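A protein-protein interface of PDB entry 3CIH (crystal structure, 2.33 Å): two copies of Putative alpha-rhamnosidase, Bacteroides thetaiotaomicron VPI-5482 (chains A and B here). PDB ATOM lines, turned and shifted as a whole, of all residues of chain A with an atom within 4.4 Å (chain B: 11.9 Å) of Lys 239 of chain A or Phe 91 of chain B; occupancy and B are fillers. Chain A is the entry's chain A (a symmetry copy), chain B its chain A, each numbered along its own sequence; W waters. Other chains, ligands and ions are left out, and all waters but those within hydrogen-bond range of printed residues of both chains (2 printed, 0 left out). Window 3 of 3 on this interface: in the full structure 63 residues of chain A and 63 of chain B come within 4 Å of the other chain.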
ATOM      1  N   ARG A  42       4.989  21.184  19.601  1.00  0.00           N
ATOM      2  CA  ARG A  42       4.006  21.852  20.434  1.00  0.00           C
ATOM      3  C   ARG A  42       2.655  22.057  19.746  1.00  0.00           C
ATOM      4  O   ARG A  42       2.126  23.169  19.706  1.00  0.00           O
ATOM      5  CB  ARG A  42       4.563  23.187  20.921  1.00  0.00           C
ATOM      6  CG  ARG A  42       5.801  23.035  21.784  1.00  0.00           C
ATOM      7  CD  ARG A  42       6.300  24.387  22.243  1.00  0.00           C
ATOM      8  NE  ARG A  42       5.338  25.048  23.121  1.00  0.00           N
ATOM      9  CZ  ARG A  42       5.108  24.688  24.378  1.00  0.00           C
ATOM     10  NH1 ARG A  42       5.762  23.670  24.911  1.00  0.00           N
ATOM     11  NH2 ARG A  42       4.229  25.353  25.108  1.00  0.00           N
ATOM     12  N   GLY A  43       2.105  20.974  19.201  1.00  0.00           N
ATOM     13  CA  GLY A  43       0.799  21.036  18.573  1.00  0.00           C
ATOM     14  C   GLY A  43       0.699  21.475  17.131  1.00  0.00           C
ATOM     15  O   GLY A  43      -0.403  21.544  16.580  1.00  0.00           O
ATOM     16  N   ILE A 217      -8.480  19.506  28.708  1.00  0.00           N
ATOM     17  CA  ILE A 217      -7.569  18.480  29.201  1.00  0.00           C
ATOM     18  C   ILE A 217      -6.276  18.703  28.417  1.00  0.00           C
ATOM     19  O   ILE A 217      -6.287  18.710  27.189  1.00  0.00           O
ATOM     20  CB  ILE A 217      -8.088  17.056  28.914  1.00  0.00           C
ATOM     21  CG1 ILE A 217      -9.399  16.813  29.669  1.00  0.00           C
ATOM     22  CG2 ILE A 217      -7.036  16.029  29.337  1.00  0.00           C
ATOM     23  CD1 ILE A 217     -10.040  15.461  29.380  1.00  0.00           C
ATOM     24  N   ASP A 218      -5.167  18.904  29.121  1.00  0.00           N
ATOM     25  CA  ASP A 218      -3.889  19.138  28.458  1.00  0.00           C
ATOM     26  C   ASP A 218      -2.842  18.065  28.716  1.00  0.00           C
ATOM     27  O   ASP A 218      -2.616  17.661  29.857  1.00  0.00           O
ATOM     28  CB  ASP A 218      -3.327  20.499  28.867  1.00  0.00           C
ATOM     29  CG  ASP A 218      -4.241  21.629  28.491  1.00  0.00           C
ATOM     30  OD1 ASP A 218      -4.734  21.627  27.349  1.00  0.00           O
ATOM     31  OD2 ASP A 218      -4.468  22.526  29.325  1.00  0.00           O
ATOM     32  N   TYR A 220       1.220  16.893  28.161  1.00  0.00           N
ATOM     33  CA  TYR A 220       2.575  17.408  27.955  1.00  0.00           C
ATOM     34  C   TYR A 220       3.505  16.200  28.005  1.00  0.00           C
ATOM     35  O   TYR A 220       3.604  15.531  29.030  1.00  0.00           O
ATOM     36  CB  TYR A 220       2.940  18.409  29.056  1.00  0.00           C
ATOM     37  CG  TYR A 220       2.037  19.622  29.095  1.00  0.00           C
ATOM     38  CD1 TYR A 220       2.237  20.698  28.226  1.00  0.00           C
ATOM     39  CD2 TYR A 220       0.966  19.681  29.986  1.00  0.00           C
ATOM     40  CE1 TYR A 220       1.392  21.805  28.244  1.00  0.00           C
ATOM     41  CE2 TYR A 220       0.109  20.780  30.015  1.00  0.00           C
ATOM     42  CZ  TYR A 220       0.330  21.839  29.145  1.00  0.00           C
ATOM     43  OH  TYR A 220      -0.493  22.935  29.193  1.00  0.00           O
ATOM     44  N   LEU A 237       3.037  18.142  22.718  1.00  0.00           N
ATOM     45  CA  LEU A 237       1.890  18.207  23.612  1.00  0.00           C
ATOM     46  C   LEU A 237       0.556  18.044  22.854  1.00  0.00           C
ATOM     47  O   LEU A 237       0.530  17.923  21.627  1.00  0.00           O
ATOM     48  CB  LEU A 237       1.910  19.550  24.343  1.00  0.00           C
ATOM     49  CG  LEU A 237       2.021  20.814  23.472  1.00  0.00           C
ATOM     50  CD1 LEU A 237       0.718  21.044  22.721  1.00  0.00           C
ATOM     51  CD2 LEU A 237       2.346  22.031  24.346  1.00  0.00           C
ATOM     52  N   ASP A 238      -0.545  18.039  23.600  1.00  0.00           N
ATOM     53  CA  ASP A 238      -1.884  17.917  23.025  1.00  0.00           C
ATOM     54  C   ASP A 238      -2.869  18.700  23.893  1.00  0.00           C
ATOM     55  O   ASP A 238      -2.630  18.917  25.086  1.00  0.00           O
ATOM     56  CB  ASP A 238      -2.328  16.446  22.957  1.00  0.00           C
ATOM     57  CG  ASP A 238      -1.641  15.660  21.829  1.00  0.00           C
ATOM     58  OD1 ASP A 238      -1.760  16.072  20.652  1.00  0.00           O
ATOM     59  OD2 ASP A 238      -0.992  14.627  22.118  1.00  0.00           O
ATOM     60  N   LYS A 239      -3.973  19.123  23.293  1.00  0.00           N
ATOM     61  CA  LYS A 239      -4.984  19.872  24.017  1.00  0.00           C
ATOM     62  C   LYS A 239      -6.358  19.379  23.597  1.00  0.00           C
ATOM     63  O   LYS A 239      -6.730  19.463  22.430  1.00  0.00           O
ATOM     64  CB  LYS A 239      -4.816  21.369  23.744  1.00  0.00           C
ATOM     65  CG  LYS A 239      -3.459  21.890  24.207  1.00  0.00           C
ATOM     66  CD  LYS A 239      -3.358  23.400  24.111  1.00  0.00           C
ATOM     67  CE  LYS A 239      -2.075  23.905  24.761  1.00  0.00           C
ATOM     68  NZ  LYS A 239      -1.974  23.526  26.204  1.00  0.00           N
ATOM     69  N   LEU A 240      -7.109  18.858  24.560  1.00  0.00           N
ATOM     70  CA  LEU A 240      -8.433  18.315  24.283  1.00  0.00           C
ATOM     71  C   LEU A 240      -9.556  19.059  24.996  1.00  0.00           C
ATOM     72  O   LEU A 240      -9.337  19.719  26.015  1.00  0.00           O
ATOM     73  CB  LEU A 240      -8.467  16.842  24.692  1.00  0.00           C
ATOM     74  CG  LEU A 240      -7.229  16.017  24.327  1.00  0.00           C
ATOM     75  CD1 LEU A 240      -7.365  14.633  24.918  1.00  0.00           C
ATOM     76  CD2 LEU A 240      -7.053  15.945  22.813  1.00  0.00           C
ATOM     77  N   THR A 248     -12.847  16.504  21.865  1.00  0.00           N
ATOM     78  CA  THR A 248     -12.237  17.051  20.664  1.00  0.00           C
ATOM     79  C   THR A 248     -10.749  17.327  20.779  1.00  0.00           C
ATOM     80  O   THR A 248     -10.291  17.895  21.770  1.00  0.00           O
ATOM     81  CB  THR A 248     -12.927  18.366  20.262  1.00  0.00           C
ATOM     82  OG1 THR A 248     -14.306  18.108  19.968  1.00  0.00           O
ATOM     83  CG2 THR A 248     -12.249  18.981  19.037  1.00  0.00           C
ATOM     84  N   ASP A 249      -9.994  16.909  19.766  1.00  0.00           N
ATOM     85  CA  ASP A 249      -8.562  17.172  19.735  1.00  0.00           C
ATOM     86  C   ASP A 249      -8.486  18.580  19.146  1.00  0.00           C
ATOM     87  O   ASP A 249      -8.791  18.783  17.974  1.00  0.00           O
ATOM     88  CB  ASP A 249      -7.844  16.185  18.816  1.00  0.00           C
ATOM     89  CG  ASP A 249      -6.340  16.405  18.790  1.00  0.00           C
ATOM     90  OD1 ASP A 249      -5.915  17.579  18.672  1.00  0.00           O
ATOM     91  OD2 ASP A 249      -5.584  15.410  18.883  1.00  0.00           O
ATOM     92  N   LEU A 250      -8.095  19.551  19.965  1.00  0.00           N
ATOM     93  CA  LEU A 250      -8.031  20.935  19.518  1.00  0.00           C
ATOM     94  C   LEU A 250      -6.955  21.245  18.475  1.00  0.00           C
ATOM     95  O   LEU A 250      -7.136  22.123  17.633  1.00  0.00           O
ATOM     96  CB  LEU A 250      -7.873  21.853  20.732  1.00  0.00           C
ATOM     97  CG  LEU A 250      -9.006  21.767  21.773  1.00  0.00           C
ATOM     98  CD1 LEU A 250      -8.665  22.641  22.967  1.00  0.00           C
ATOM     99  CD2 LEU A 250     -10.335  22.207  21.166  1.00  0.00           C
ATOM    100  N   ALA A 251      -5.842  20.528  18.523  1.00  0.00           N
ATOM    101  CA  ALA A 251      -4.764  20.763  17.575  1.00  0.00           C
ATOM    102  C   ALA A 251      -5.187  20.464  16.139  1.00  0.00           C
ATOM    103  O   ALA A 251      -4.866  21.222  15.222  1.00  0.00           O
ATOM    104  CB  ALA A 251      -3.546  19.916  17.947  1.00  0.00           C
ATOM    105  N   ILE B  75      -8.188  32.836   8.492  1.00  0.00           N
ATOM    106  CA  ILE B  75      -7.418  31.891   7.702  1.00  0.00           C
ATOM    107  C   ILE B  75      -8.208  30.640   7.387  1.00  0.00           C
ATOM    108  O   ILE B  75      -8.753  30.002   8.278  1.00  0.00           O
ATOM    109  CB  ILE B  75      -6.126  31.467   8.438  1.00  0.00           C
ATOM    110  CG1 ILE B  75      -5.251  32.692   8.704  1.00  0.00           C
ATOM    111  CG2 ILE B  75      -5.351  30.448   7.604  1.00  0.00           C
ATOM    112  CD1 ILE B  75      -4.105  32.428   9.669  1.00  0.00           C
ATOM    113  N   THR B  80      -4.011  20.037   5.265  1.00  0.00           N
ATOM    114  CA  THR B  80      -3.472  20.149   6.618  1.00  0.00           C
ATOM    115  C   THR B  80      -2.474  21.296   6.579  1.00  0.00           C
ATOM    116  O   THR B  80      -1.726  21.437   5.609  1.00  0.00           O
ATOM    117  CB  THR B  80      -2.741  18.865   7.016  1.00  0.00           C
ATOM    118  OG1 THR B  80      -3.684  17.794   7.074  1.00  0.00           O
ATOM    119  CG2 THR B  80      -2.052  19.021   8.362  1.00  0.00           C
ATOM    120  N   TYR B  81      -2.440  22.117   7.619  1.00  0.00           N
ATOM    121  CA  TYR B  81      -1.516  23.237   7.589  1.00  0.00           C
ATOM    122  C   TYR B  81      -1.022  23.695   8.945  1.00  0.00           C
ATOM    123  O   TYR B  81      -1.524  23.267   9.983  1.00  0.00           O
ATOM    124  CB  TYR B  81      -2.181  24.413   6.858  1.00  0.00           C
ATOM    125  CG  TYR B  81      -3.308  25.089   7.620  1.00  0.00           C
ATOM    126  CD1 TYR B  81      -3.047  26.141   8.509  1.00  0.00           C
ATOM    127  CD2 TYR B  81      -4.634  24.678   7.462  1.00  0.00           C
ATOM    128  CE1 TYR B  81      -4.075  26.765   9.218  1.00  0.00           C
ATOM    129  CE2 TYR B  81      -5.675  25.295   8.166  1.00  0.00           C
ATOM    130  CZ  TYR B  81      -5.382  26.342   9.045  1.00  0.00           C
ATOM    131  OH  TYR B  81      -6.382  26.978   9.749  1.00  0.00           O
ATOM    132  N   ASN B  82       0.005  24.543   8.920  1.00  0.00           N
ATOM    133  CA  ASN B  82       0.542  25.140  10.133  1.00  0.00           C
ATOM    134  C   ASN B  82       0.678  26.628   9.853  1.00  0.00           C
ATOM    135  O   ASN B  82       0.560  27.062   8.704  1.00  0.00           O
ATOM    136  CB  ASN B  82       1.893  24.525  10.564  1.00  0.00           C
ATOM    137  CG  ASN B  82       3.023  24.756   9.563  1.00  0.00           C
ATOM    138  OD1 ASN B  82       3.059  25.753   8.852  1.00  0.00           O
ATOM    139  ND2 ASN B  82       3.973  23.832   9.539  1.00  0.00           N
ATOM    140  N   VAL B  83       0.886  27.414  10.900  1.00  0.00           N
ATOM    141  CA  VAL B  83       1.021  28.856  10.740  1.00  0.00           C
ATOM    142  C   VAL B  83       2.228  29.319  11.525  1.00  0.00           C
ATOM    143  O   VAL B  83       2.345  29.048  12.718  1.00  0.00           O
ATOM    144  CB  VAL B  83      -0.226  29.610  11.257  1.00  0.00           C
ATOM    145  CG1 VAL B  83       0.006  31.109  11.176  1.00  0.00           C
ATOM    146  CG2 VAL B  83      -1.447  29.226  10.443  1.00  0.00           C
ATOM    147  N   LYS B  84       3.132  30.013  10.850  1.00  0.00           N
ATOM    148  CA  LYS B  84       4.340  30.499  11.503  1.00  0.00           C
ATOM    149  C   LYS B  84       4.413  32.013  11.388  1.00  0.00           C
ATOM    150  O   LYS B  84       4.313  32.561  10.293  1.00  0.00           O
ATOM    151  CB  LYS B  84       5.577  29.868  10.860  1.00  0.00           C
ATOM    152  CG  LYS B  84       6.879  30.213  11.559  1.00  0.00           C
ATOM    153  CD  LYS B  84       8.088  29.970  10.661  1.00  0.00           C
ATOM    154  CE  LYS B  84       8.281  28.504  10.352  1.00  0.00           C
ATOM    155  NZ  LYS B  84       9.473  28.301   9.485  1.00  0.00           N
ATOM    156  N   LEU B  85       4.561  32.687  12.523  1.00  0.00           N
ATOM    157  CA  LEU B  85       4.660  34.144  12.542  1.00  0.00           C
ATOM    158  C   LEU B  85       6.027  34.488  13.112  1.00  0.00           C
ATOM    159  O   LEU B  85       6.336  34.160  14.265  1.00  0.00           O
ATOM    160  CB  LEU B  85       3.551  34.754  13.407  1.00  0.00           C
ATOM    161  CG  LEU B  85       3.536  36.279  13.583  1.00  0.00           C
ATOM    162  CD1 LEU B  85       3.295  36.982  12.246  1.00  0.00           C
ATOM    163  CD2 LEU B  85       2.438  36.652  14.581  1.00  0.00           C
ATOM    164  N   ASP B  86       6.855  35.122  12.286  1.00  0.00           N
ATOM    165  CA  ASP B  86       8.206  35.501  12.684  1.00  0.00           C
ATOM    166  C   ASP B  86       8.988  34.315  13.233  1.00  0.00           C
ATOM    167  O   ASP B  86       9.641  34.417  14.269  1.00  0.00           O
ATOM    168  CB  ASP B  86       8.164  36.622  13.733  1.00  0.00           C
ATOM    169  CG  ASP B  86       7.276  37.777  13.313  1.00  0.00           C
ATOM    170  OD1 ASP B  86       7.249  38.089  12.108  1.00  0.00           O
ATOM    171  OD2 ASP B  86       6.613  38.376  14.183  1.00  0.00           O
ATOM    172  N   GLY B  87       8.910  33.184  12.539  1.00  0.00           N
ATOM    173  CA  GLY B  87       9.635  31.998  12.965  1.00  0.00           C
ATOM    174  C   GLY B  87       8.998  31.168  14.066  1.00  0.00           C
ATOM    175  O   GLY B  87       9.506  30.096  14.407  1.00  0.00           O
ATOM    176  N   LYS B  88       7.884  31.643  14.618  1.00  0.00           N
ATOM    177  CA  LYS B  88       7.215  30.923  15.697  1.00  0.00           C
ATOM    178  C   LYS B  88       5.958  30.152  15.281  1.00  0.00           C
ATOM    179  O   LYS B  88       4.944  30.744  14.889  1.00  0.00           O
ATOM    180  CB  LYS B  88       6.870  31.893  16.835  1.00  0.00           C
ATOM    181  CG  LYS B  88       6.219  31.228  18.052  1.00  0.00           C
ATOM    182  CD  LYS B  88       7.125  30.166  18.683  1.00  0.00           C
ATOM    183  CE  LYS B  88       6.441  29.455  19.859  1.00  0.00           C
ATOM    184  NZ  LYS B  88       7.306  28.432  20.534  1.00  0.00           N
ATOM    185  N   LEU B  89       6.039  28.826  15.386  1.00  0.00           N
ATOM    186  CA  LEU B  89       4.927  27.946  15.047  1.00  0.00           C
ATOM    187  C   LEU B  89       3.754  28.129  16.007  1.00  0.00           C
ATOM    188  O   LEU B  89       3.916  27.991  17.219  1.00  0.00           O
ATOM    189  CB  LEU B  89       5.370  26.483  15.092  1.00  0.00           C
ATOM    190  CG  LEU B  89       6.072  25.882  13.878  1.00  0.00           C
ATOM    191  CD1 LEU B  89       6.511  24.459  14.197  1.00  0.00           C
ATOM    192  CD2 LEU B  89       5.127  25.897  12.679  1.00  0.00           C
ATOM    193  N   GLN B  90       2.581  28.447  15.461  1.00  0.00           N
ATOM    194  CA  GLN B  90       1.381  28.614  16.272  1.00  0.00           C
ATOM    195  C   GLN B  90       0.831  27.223  16.602  1.00  0.00           C
ATOM    196  O   GLN B  90       1.216  26.227  15.986  1.00  0.00           O
ATOM    197  CB  GLN B  90       0.314  29.402  15.510  1.00  0.00           C
ATOM    198  CG  GLN B  90       0.721  30.797  15.047  1.00  0.00           C
ATOM    199  CD  GLN B  90       1.251  31.673  16.173  1.00  0.00           C
ATOM    200  OE1 GLN B  90       2.465  31.841  16.327  1.00  0.00           O
ATOM    201  NE2 GLN B  90       0.346  32.233  16.965  1.00  0.00           N
ATOM    202  N   PHE B  91      -0.072  27.157  17.571  1.00  0.00           N
ATOM    203  CA  PHE B  91      -0.664  25.884  17.946  1.00  0.00           C
ATOM    204  C   PHE B  91      -1.700  25.457  16.906  1.00  0.00           C
ATOM    205  O   PHE B  91      -2.421  26.289  16.373  1.00  0.00           O
ATOM    206  CB  PHE B  91      -1.346  25.996  19.316  1.00  0.00           C
ATOM    207  CG  PHE B  91      -2.062  24.741  19.737  1.00  0.00           C
ATOM    208  CD1 PHE B  91      -1.366  23.698  20.347  1.00  0.00           C
ATOM    209  CD2 PHE B  91      -3.429  24.591  19.498  1.00  0.00           C
ATOM    210  CE1 PHE B  91      -2.027  22.520  20.714  1.00  0.00           C
ATOM    211  CE2 PHE B  91      -4.100  23.423  19.858  1.00  0.00           C
ATOM    212  CZ  PHE B  91      -3.402  22.384  20.467  1.00  0.00           C
ATOM    213  N   GLY B  92      -1.751  24.156  16.629  1.00  0.00           N
ATOM    214  CA  GLY B  92      -2.708  23.592  15.692  1.00  0.00           C
ATOM    215  C   GLY B  92      -2.955  24.273  14.358  1.00  0.00           C
ATOM    216  O   GLY B  92      -2.024  24.635  13.636  1.00  0.00           O
ATOM    217  N   MET B  93      -4.233  24.411  14.019  1.00  0.00           N
ATOM    218  CA  MET B  93      -4.634  25.050  12.771  1.00  0.00           C
ATOM    219  C   MET B  93      -5.577  26.200  13.082  1.00  0.00           C
ATOM    220  O   MET B  93      -6.798  26.063  13.011  1.00  0.00           O
ATOM    221  CB  MET B  93      -5.310  24.038  11.832  1.00  0.00           C
ATOM    222  CG  MET B  93      -4.369  22.940  11.371  1.00  0.00           C
ATOM    223  SD  MET B  93      -5.225  21.728  10.099  1.00  0.00           S
ATOM    224  CE  MET B  93      -5.620  20.164  11.248  1.00  0.00           C
ATOM    225  N   PRO B  94      -5.016  27.358  13.443  1.00  0.00           N
ATOM    226  CA  PRO B  94      -5.839  28.521  13.767  1.00  0.00           C
ATOM    227  C   PRO B  94      -6.621  29.080  12.583  1.00  0.00           C
ATOM    228  O   PRO B  94      -6.131  29.103  11.452  1.00  0.00           O
ATOM    229  CB  PRO B  94      -4.820  29.515  14.318  1.00  0.00           C
ATOM    230  CG  PRO B  94      -3.573  29.171  13.569  1.00  0.00           C
ATOM    231  CD  PRO B  94      -3.583  27.665  13.591  1.00  0.00           C
ATOM    232  N   GLU B  95      -7.845  29.530  12.855  1.00  0.00           N
ATOM    233  CA  GLU B  95      -8.692  30.113  11.824  1.00  0.00           C
ATOM    234  C   GLU B  95      -8.573  31.636  11.834  1.00  0.00           C
ATOM    235  O   GLU B  95      -9.074  32.313  10.936  1.00  0.00           O
ATOM    236  CB  GLU B  95     -10.146  29.706  12.028  1.00  0.00           C
ATOM    237  CG  GLU B  95     -10.423  28.229  11.802  1.00  0.00           C
ATOM    238  CD  GLU B  95     -11.909  27.905  11.872  1.00  0.00           C
ATOM    239  OE1 GLU B  95     -12.665  28.311  10.954  1.00  0.00           O
ATOM    240  OE2 GLU B  95     -12.319  27.253  12.860  1.00  0.00           O
ATOM    241  N   THR B  96      -7.928  32.170  12.865  1.00  0.00           N
ATOM    242  CA  THR B  96      -7.705  33.609  12.983  1.00  0.00           C
ATOM    243  C   THR B  96      -6.379  33.821  13.697  1.00  0.00           C
ATOM    244  O   THR B  96      -5.975  32.999  14.511  1.00  0.00           O
ATOM    245  CB  THR B  96      -8.807  34.306  13.793  1.00  0.00           C
ATOM    246  OG1 THR B  96      -8.773  33.840  15.148  1.00  0.00           O
ATOM    247  CG2 THR B  96     -10.171  34.018  13.189  1.00  0.00           C
ATOM    248  N   LEU B  97      -5.706  34.921  13.386  1.00  0.00           N
ATOM    249  CA  LEU B  97      -4.425  35.233  14.006  1.00  0.00           C
ATOM    250  C   LEU B  97      -4.288  36.746  14.139  1.00  0.00           C
ATOM    251  O   LEU B  97      -4.587  37.479  13.194  1.00  0.00           O
ATOM    252  CB  LEU B  97      -3.273  34.680  13.150  1.00  0.00           C
ATOM    253  CG  LEU B  97      -1.836  34.962  13.598  1.00  0.00           C
ATOM    254  CD1 LEU B  97      -1.544  34.217  14.889  1.00  0.00           C
ATOM    255  CD2 LEU B  97      -0.858  34.528  12.505  1.00  0.00           C
ATOM    256  N   LEU B  98      -3.854  37.215  15.305  1.00  0.00           N
ATOM    257  CA  LEU B  98      -3.676  38.652  15.494  1.00  0.00           C
ATOM    258  C   LEU B  98      -2.274  39.037  15.041  1.00  0.00           C
ATOM    259  O   LEU B  98      -1.285  38.452  15.483  1.00  0.00           O
ATOM    260  CB  LEU B  98      -3.872  39.066  16.962  1.00  0.00           C
ATOM    261  CG  LEU B  98      -3.560  40.553  17.213  1.00  0.00           C
ATOM    262  CD1 LEU B  98      -4.571  41.420  16.467  1.00  0.00           C
ATOM    263  CD2 LEU B  98      -3.591  40.871  18.696  1.00  0.00           C
ATOM    264  N   LEU B 106       4.671  36.282   7.771  1.00  0.00           N
ATOM    265  CA  LEU B 106       3.615  35.284   7.913  1.00  0.00           C
ATOM    266  C   LEU B 106       3.887  34.111   6.954  1.00  0.00           C
ATOM    267  O   LEU B 106       3.981  34.299   5.742  1.00  0.00           O
ATOM    268  CB  LEU B 106       2.259  35.929   7.599  1.00  0.00           C
ATOM    269  CG  LEU B 106       1.003  35.061   7.719  1.00  0.00           C
ATOM    270  CD1 LEU B 106       0.885  34.515   9.134  1.00  0.00           C
ATOM    271  CD2 LEU B 106      -0.223  35.882   7.371  1.00  0.00           C
ATOM    272  N   ASN B 107       4.005  32.906   7.505  1.00  0.00           N
ATOM    273  CA  ASN B 107       4.282  31.719   6.706  1.00  0.00           C
ATOM    274  C   ASN B 107       3.270  30.611   6.979  1.00  0.00           C
ATOM    275  O   ASN B 107       3.094  30.171   8.117  1.00  0.00           O
ATOM    276  CB  ASN B 107       5.700  31.200   6.989  1.00  0.00           C
ATOM    277  CG  ASN B 107       6.767  32.249   6.733  1.00  0.00           C
ATOM    278  OD1 ASN B 107       6.732  33.333   7.308  1.00  0.00           O
ATOM    279  ND2 ASN B 107       7.724  31.928   5.870  1.00  0.00           N
ATOM    280  N   ILE B 108       2.619  30.153   5.920  1.00  0.00           N
ATOM    281  CA  ILE B 108       1.623  29.108   6.044  1.00  0.00           C
ATOM    282  C   ILE B 108       1.977  27.943   5.125  1.00  0.00           C
ATOM    283  O   ILE B 108       1.900  28.060   3.908  1.00  0.00           O
ATOM    284  CB  ILE B 108       0.223  29.684   5.718  1.00  0.00           C
ATOM    285  CG1 ILE B 108      -0.050  30.866   6.651  1.00  0.00           C
ATOM    286  CG2 ILE B 108      -0.855  28.614   5.868  1.00  0.00           C
ATOM    287  CD1 ILE B 108      -1.332  31.583   6.396  1.00  0.00           C
ATOM    288  N   LYS B 109       2.383  26.825   5.719  1.00  0.00           N
ATOM    289  CA  LYS B 109       2.762  25.634   4.956  1.00  0.00           C
ATOM    290  C   LYS B 109       1.590  24.652   4.930  1.00  0.00           C
ATOM    291  O   LYS B 109       1.077  24.250   5.979  1.00  0.00           O
ATOM    292  CB  LYS B 109       3.998  24.993   5.593  1.00  0.00           C
ATOM    293  CG  LYS B 109       4.810  24.089   4.684  1.00  0.00           C
ATOM    294  CD  LYS B 109       6.221  23.947   5.247  1.00  0.00           C
ATOM    295  CE  LYS B 109       7.147  23.195   4.307  1.00  0.00           C
ATOM    296  NZ  LYS B 109       8.551  23.207   4.820  1.00  0.00           N
HETATM  297  O   HOH W   1      -6.460  24.331  16.095  1.00  0.00           O
HETATM  298  O   HOH W   2       4.688  27.491  21.585  1.00  0.00           O
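Phe 91 of chain B touches Arg 42 of chain A. CA of Gly 43 of chain A touches CE1 of Phe 91 of chain B, at 3.8 Å. Phe 91 of chain B touches Leu 237 of chain A (CE1 to CD1, 3.7 Å). Lys 239 of chain A touches Phe 91 of chain B. Leu 250 of chain A touches Phe 91 of chain B (C to CE2, 3.8 Å). CB of Ala 251 of chain A touches CZ of Phe 91 of chain B, at 3.5 Å. Ala 251 of chain A touches Gly 92 of chain B.
Water W1 bridges O of Leu 250 of chain A (2.8 Å) and N of Met 93 of chain B (3.0 Å). Water W2 bridges NE of Arg 42 of chain A (3.0 Å) and NZ of Lys 88 of chain B (3.0 Å).
No position is printed for both chains. Of the 9 pairs that touch across the chains among the printed residues, none has its exchanged pair printed and touching as well.
The backbone carbonyl oxygen (O) of Met 93 of chain B lies within hydrogen-bond range of the side-chain hydroxyl (OH) of Tyr 81 of chain B (3.4 Å). The side-chain amino group (NZ) of Lys 239 of chain A is in salt-bridge range of the side-chain carboxylate (OD1) of Asp 218 of chain A (3.5 Å). The side-chain hydroxyl (OH) of Tyr 220 of chain A sits at hydrogen-bond distance from the side-chain amino group (NZ) of Lys 239 of chain A, 3.4 Å away. The backbone carbonyl oxygen of Lys 239 of chain A lies within hydrogen-bond range of the backbone NH of Leu 250 of chain A, 2.8 Å away. OD1 of Asp 249 of chain A is in hydrogen-bond range of N of Ala 251 of chain A (3.0 Å).
O of Gly 43 of chain A lies within hydrogen-bond range of N of Gly 92 of chain B, 2.9 Å away. The backbone NH (N) of Met 93 of chain B lies within hydrogen-bond range of the backbone carbonyl oxygen (O) of Ala 251 of chain A.
Of the printed residues of chain B, Arg 42 of chain A touches Phe 91 (3.6 Å). Of chain B, only Phe 91 and Gly 92 come within 4 Å of Gly 43 of chain A. No residue of chain B comes within 4 Å of Asp 218 of chain A. Of chain B, only Phe 91 comes within 4 Å of Leu 237 of chain A. No residue of chain B comes within 4 Å of Asp 238 of chain A. Lys 239 of chain A touches just one residue of chain B: Phe 91 (3.7 Å). No residue of chain B comes within 4 Å of Leu 240 of chain A. Leu 250 of chain A touches just one residue of chain B: Phe 91 (3.8 Å). Thr 80 of chain B touches none of the printed residues of chain A. Of chain A, only Arg 42 (3.6 Å), Gly 43 (3.8 Å), Leu 237 (3.7 Å), Lys 239 (3.7 Å), Leu 250 (3.8 Å) and Ala 251 (3.5 Å) come within 4 Å of Phe 91 of chain B. Of the printed residues of chain A, Gly 92 of chain B touches Gly 43 (2.9 Å) and Ala 251 (3.2 Å). Printed residues of chain A within 4 Å of Met 93 of chain B: Ala 251. The nearest residue of chain B that does not touch Lys 239 of chain A is Gly 92 of chain B (7.7 Å). The nearest printed residue of chain A that does not touch Phe 91 of chain B is Asp 238 of chain A (5.0 Å). The nearest printed residue of chain A that does not touch Gly 92 of chain B is Arg 42 of chain A (5.0 Å).
Hydrophobic or aromatic side chains of chain B within 4 Å of the printed part of chain A: Phe 91. Hydrophobic or aromatic side chains of chain A within 4 Å of the printed part of chain B: Leu 237 and Ala 251. Along chain A the printed residues that touch a printed residue of chain B span positions 42 to 251. Among the printed residues, no Asp or Glu carboxylate lies within 4 Å of a Lys or Arg side-chain nitrogen of the other chain.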
